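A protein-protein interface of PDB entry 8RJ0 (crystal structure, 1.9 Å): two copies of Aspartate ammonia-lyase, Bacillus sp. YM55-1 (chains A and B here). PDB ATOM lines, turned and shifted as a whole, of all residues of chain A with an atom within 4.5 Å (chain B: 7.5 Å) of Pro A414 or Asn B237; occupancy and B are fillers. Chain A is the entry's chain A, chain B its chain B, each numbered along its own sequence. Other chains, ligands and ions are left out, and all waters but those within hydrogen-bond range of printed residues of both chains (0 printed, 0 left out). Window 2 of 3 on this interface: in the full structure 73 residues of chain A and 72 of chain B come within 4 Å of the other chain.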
ATOM      1  N   THR A 410       9.996  -8.601   9.710  1.00  0.00           N
ATOM      2  CA  THR A 410       9.210  -9.689  10.254  1.00  0.00           C
ATOM      3  C   THR A 410       9.548  -9.894  11.722  1.00  0.00           C
ATOM      4  O   THR A 410       8.704 -10.306  12.505  1.00  0.00           O
ATOM      5  CB  THR A 410       9.511 -10.914   9.370  1.00  0.00           C
ATOM      6  OG1 THR A 410       8.827 -10.628   8.143  1.00  0.00           O
ATOM      7  CG2 THR A 410       9.020 -12.234   9.930  1.00  0.00           C
ATOM      8  N   ALA A 411      10.813  -9.690  12.097  1.00  0.00           N
ATOM      9  CA  ALA A 411      11.223  -9.823  13.490  1.00  0.00           C
ATOM     10  C   ALA A 411      10.600  -8.709  14.358  1.00  0.00           C
ATOM     11  O   ALA A 411      10.294  -8.942  15.537  1.00  0.00           O
ATOM     12  CB  ALA A 411      12.732  -9.786  13.577  1.00  0.00           C
ATOM     13  N   ILE A 412      10.361  -7.523  13.775  1.00  0.00           N
ATOM     14  CA  ILE A 412       9.910  -6.392  14.599  1.00  0.00           C
ATOM     15  C   ILE A 412       8.372  -6.273  14.676  1.00  0.00           C
ATOM     16  O   ILE A 412       7.855  -5.591  15.595  1.00  0.00           O
ATOM     17  CB  ILE A 412      10.588  -5.069  14.173  1.00  0.00           C
ATOM     18  CG1 ILE A 412       9.988  -4.496  12.915  1.00  0.00           C
ATOM     19  CG2 ILE A 412      12.108  -5.241  14.040  1.00  0.00           C
ATOM     20  CD1 ILE A 412      10.622  -3.189  12.488  1.00  0.00           C
ATOM     21  N   ASN A 413       7.653  -6.943  13.750  1.00  0.00           N
ATOM     22  CA  ASN A 413       6.212  -6.786  13.585  1.00  0.00           C
ATOM     23  C   ASN A 413       5.414  -7.001  14.869  1.00  0.00           C
ATOM     24  O   ASN A 413       4.547  -6.204  15.211  1.00  0.00           O
ATOM     25  CB  ASN A 413       5.640  -7.736  12.544  1.00  0.00           C
ATOM     26  CG  ASN A 413       5.402  -6.972  11.274  1.00  0.00           C
ATOM     27  OD1 ASN A 413       6.352  -6.423  10.728  1.00  0.00           O
ATOM     28  ND2 ASN A 413       4.151  -6.839  10.855  1.00  0.00           N
ATOM     29  N   PRO A 414       5.573  -8.122  15.587  1.00  0.00           N
ATOM     30  CA  PRO A 414       4.763  -8.322  16.789  1.00  0.00           C
ATOM     31  C   PRO A 414       5.080  -7.324  17.907  1.00  0.00           C
ATOM     32  O   PRO A 414       4.318  -7.201  18.851  1.00  0.00           O
ATOM     33  CB  PRO A 414       5.069  -9.780  17.230  1.00  0.00           C
ATOM     34  CG  PRO A 414       6.318 -10.199  16.453  1.00  0.00           C
ATOM     35  CD  PRO A 414       6.548  -9.199  15.315  1.00  0.00           C
ATOM     36  N   HIS A 415       6.259  -6.689  17.866  1.00  0.00           N
ATOM     37  CA  HIS A 415       6.637  -5.697  18.870  1.00  0.00           C
ATOM     38  C   HIS A 415       5.996  -4.349  18.566  1.00  0.00           C
ATOM     39  O   HIS A 415       5.481  -3.686  19.446  1.00  0.00           O
ATOM     40  CB  HIS A 415       8.158  -5.532  18.946  1.00  0.00           C
ATOM     41  CG  HIS A 415       8.736  -6.799  19.416  1.00  0.00           C
ATOM     42  ND1 HIS A 415       9.310  -7.694  18.544  1.00  0.00           N
ATOM     43  CD2 HIS A 415       8.730  -7.363  20.637  1.00  0.00           C
ATOM     44  CE1 HIS A 415       9.677  -8.762  19.251  1.00  0.00           C
ATOM     45  NE2 HIS A 415       9.338  -8.577  20.514  1.00  0.00           N
ATOM     46  N   VAL A 416       5.994  -3.979  17.295  1.00  0.00           N
ATOM     47  CA  VAL A 416       5.668  -2.636  16.868  1.00  0.00           C
ATOM     48  C   VAL A 416       4.270  -2.556  16.245  1.00  0.00           C
ATOM     49  O   VAL A 416       3.730  -1.477  16.163  1.00  0.00           O
ATOM     50  CB  VAL A 416       6.858  -2.363  15.930  1.00  0.00           C
ATOM     51  CG1 VAL A 416       6.551  -1.559  14.669  1.00  0.00           C
ATOM     52  CG2 VAL A 416       8.023  -1.803  16.740  1.00  0.00           C
ATOM     53  N   GLY A 417       3.662  -3.696  15.864  1.00  0.00           N
ATOM     54  CA  GLY A 417       2.350  -3.725  15.231  1.00  0.00           C
ATOM     55  C   GLY A 417       2.454  -3.320  13.761  1.00  0.00           C
ATOM     56  O   GLY A 417       3.345  -2.558  13.381  1.00  0.00           O
ATOM     57  N   GLY A 463       9.092 -18.559  18.317  1.00  0.00           N
ATOM     58  CA  GLY A 463       8.892 -17.628  19.422  1.00  0.00           C
ATOM     59  C   GLY A 463       8.675 -16.211  18.886  1.00  0.00           C
ATOM     60  O   GLY A 463       8.638 -16.018  17.658  1.00  0.00           O
ATOM     61  N   LEU B  65      -5.512 -17.827  18.657  1.00  0.00           N
ATOM     62  CA  LEU B  65      -5.184 -16.958  17.518  1.00  0.00           C
ATOM     63  C   LEU B  65      -6.381 -16.763  16.593  1.00  0.00           C
ATOM     64  O   LEU B  65      -6.492 -15.766  15.889  1.00  0.00           O
ATOM     65  CB  LEU B  65      -3.984 -17.523  16.740  1.00  0.00           C
ATOM     66  CG  LEU B  65      -2.615 -17.368  17.393  1.00  0.00           C
ATOM     67  CD1 LEU B  65      -1.549 -18.175  16.649  1.00  0.00           C
ATOM     68  CD2 LEU B  65      -2.242 -15.865  17.464  1.00  0.00           C
ATOM     69  N   SER B 138      -0.968 -19.146  10.492  1.00  0.00           N
ATOM     70  CA  SER B 138       0.175 -19.782  11.142  1.00  0.00           C
ATOM     71  C   SER B 138       0.896 -20.724  10.144  1.00  0.00           C
ATOM     72  O   SER B 138       1.776 -21.471  10.521  1.00  0.00           O
ATOM     73  CB  SER B 138      -0.191 -20.536  12.416  1.00  0.00           C
ATOM     74  OG  SER B 138      -0.855 -19.738  13.384  1.00  0.00           O
ATOM     75  N   GLY B 228       5.033 -25.193  11.115  1.00  0.00           N
ATOM     76  CA  GLY B 228       5.657 -24.184  11.956  1.00  0.00           C
ATOM     77  C   GLY B 228       6.910 -23.561  11.353  1.00  0.00           C
ATOM     78  O   GLY B 228       7.460 -22.611  11.902  1.00  0.00           O
ATOM     79  N   THR B 230       7.164 -21.617   8.887  1.00  0.00           N
ATOM     80  CA  THR B 230       6.911 -20.361   8.187  1.00  0.00           C
ATOM     81  C   THR B 230       7.658 -20.335   6.834  1.00  0.00           C
ATOM     82  O   THR B 230       7.662 -21.325   6.115  1.00  0.00           O
ATOM     83  CB  THR B 230       7.095 -19.152   9.114  1.00  0.00           C
ATOM     84  OG1 THR B 230       8.416 -18.873   9.584  1.00  0.00           O
ATOM     85  CG2 THR B 230       6.289 -19.303  10.399  1.00  0.00           C
ATOM     86  N   THR B 234      12.719 -21.015   9.550  1.00  0.00           N
ATOM     87  CA  THR B 234      13.228 -20.464  10.807  1.00  0.00           C
ATOM     88  C   THR B 234      12.151 -20.547  11.871  1.00  0.00           C
ATOM     89  O   THR B 234      12.452 -20.530  13.060  1.00  0.00           O
ATOM     90  CB  THR B 234      13.723 -19.030  10.693  1.00  0.00           C
ATOM     91  OG1 THR B 234      12.650 -18.253  10.151  1.00  0.00           O
ATOM     92  CG2 THR B 234      14.944 -18.978   9.815  1.00  0.00           C
ATOM     93  N   GLY B 235      10.893 -20.569  11.447  1.00  0.00           N
ATOM     94  CA  GLY B 235       9.816 -20.608  12.414  1.00  0.00           C
ATOM     95  C   GLY B 235       9.610 -19.241  13.073  1.00  0.00           C
ATOM     96  O   GLY B 235       8.878 -19.142  14.072  1.00  0.00           O
ATOM     97  N   LEU B 236      10.234 -18.200  12.508  1.00  0.00           N
ATOM     98  CA  LEU B 236      10.198 -16.897  13.143  1.00  0.00           C
ATOM     99  C   LEU B 236       8.725 -16.501  13.272  1.00  0.00           C
ATOM    100  O   LEU B 236       7.954 -16.588  12.293  1.00  0.00           O
ATOM    101  CB  LEU B 236      11.007 -15.822  12.415  1.00  0.00           C
ATOM    102  CG  LEU B 236      10.865 -14.413  13.021  1.00  0.00           C
ATOM    103  CD1 LEU B 236      11.359 -14.345  14.483  1.00  0.00           C
ATOM    104  CD2 LEU B 236      11.476 -13.362  12.158  1.00  0.00           C
ATOM    105  N   ASN B 237       8.340 -16.174  14.522  1.00  0.00           N
ATOM    106  CA  ASN B 237       6.991 -15.724  14.859  1.00  0.00           C
ATOM    107  C   ASN B 237       5.994 -16.883  14.952  1.00  0.00           C
ATOM    108  O   ASN B 237       4.833 -16.651  15.270  1.00  0.00           O
ATOM    109  CB  ASN B 237       6.461 -14.641  13.910  1.00  0.00           C
ATOM    110  CG  ASN B 237       7.224 -13.337  14.035  1.00  0.00           C
ATOM    111  OD1 ASN B 237       7.915 -13.106  15.034  1.00  0.00           O
ATOM    112  ND2 ASN B 237       7.136 -12.480  13.031  1.00  0.00           N
ATOM    113  N   ALA B 238       6.407 -18.127  14.706  1.00  0.00           N
ATOM    114  CA  ALA B 238       5.546 -19.250  15.018  1.00  0.00           C
ATOM    115  C   ALA B 238       5.560 -19.437  16.528  1.00  0.00           C
ATOM    116  O   ALA B 238       6.558 -19.232  17.220  1.00  0.00           O
ATOM    117  CB  ALA B 238       5.962 -20.525  14.306  1.00  0.00           C
ATOM    118  N   ASP B 239       4.408 -19.843  17.017  1.00  0.00           N
ATOM    119  CA  ASP B 239       4.236 -20.172  18.402  1.00  0.00           C
ATOM    120  C   ASP B 239       4.555 -21.642  18.587  1.00  0.00           C
ATOM    121  O   ASP B 239       3.834 -22.523  18.097  1.00  0.00           O
ATOM    122  CB  ASP B 239       2.838 -19.720  18.777  1.00  0.00           C
ATOM    123  CG  ASP B 239       2.373 -20.223  20.126  1.00  0.00           C
ATOM    124  OD1 ASP B 239       3.181 -20.873  20.797  1.00  0.00           O
ATOM    125  OD2 ASP B 239       1.221 -19.939  20.481  1.00  0.00           O
ATOM    126  N   PRO B 240       5.576 -21.980  19.409  1.00  0.00           N
ATOM    127  CA  PRO B 240       5.877 -23.370  19.722  1.00  0.00           C
ATOM    128  C   PRO B 240       4.697 -24.183  20.242  1.00  0.00           C
ATOM    129  O   PRO B 240       4.615 -25.374  20.001  1.00  0.00           O
ATOM    130  CB  PRO B 240       7.042 -23.255  20.744  1.00  0.00           C
ATOM    131  CG  PRO B 240       7.686 -21.939  20.393  1.00  0.00           C
ATOM    132  CD  PRO B 240       6.500 -21.046  20.094  1.00  0.00           C
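O of Thr A410 is in hydrogen-bond range of ND2 of Asn B237 (2.7 Å). N of Gly A463 lies within hydrogen-bond range of O of Ala B238 (2.8 Å). O of Gly A463 is in hydrogen-bond range of N of Asn B237, at 3.2 Å.
OG1 of Thr B234 sits close to N of Leu B236 (3.4 Å). O of Ala A411 is in hydrogen-bond range of ND1 of His A415 (3.4 Å).
Thr A410 touches Leu B236 (CG2 to CD2, 3.5 Å). Leu B236 touches Ala A411 (CD2 to N, 3.7 Å). OD1 of Asn B237 touches CG of Pro A414 (3.6 Å).
Pro A414 touches just one residue of chain B: Asn B237. Of chain A, only Thr A410 (2.7 Å), Pro A414 (3.6 Å) and Gly A463 (3.2 Å) come within 4 Å of Asn B237. Of the printed residues of chain A, Ala B238 touches Gly A463. Printed residues of chain B within 4 Å of Ala A411: Leu B236 (3.7 Å). Printed residues of chain B within 4 Å of Thr A410: Leu B236 (3.5 Å) and Asn B237 (2.7 Å). Printed residues of chain A within 4 Å of Leu B236: Thr A410 and Ala A411. Thr B230 touches none of the printed residues of chain A. The nearest residue of chain B that does not touch Pro A414 is Leu B236 (6.8 Å). The nearest printed residue of chain A that does not touch Asn B237 is Ala A411 (4.7 Å).
Printed residues of chain B that touch a printed residue of chain A: Leu B236, Asn B237 and Ala B238. Hydrophobic or aromatic side chains of chain A within 4 Å of the printed part of chain B: Pro A414. Among the printed residues, 6 pairs touch across the chains.
No position is printed for both chains. Of the 6 pairs that touch across the chains among the printed residues, none has its exchanged pair printed and touching as well.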
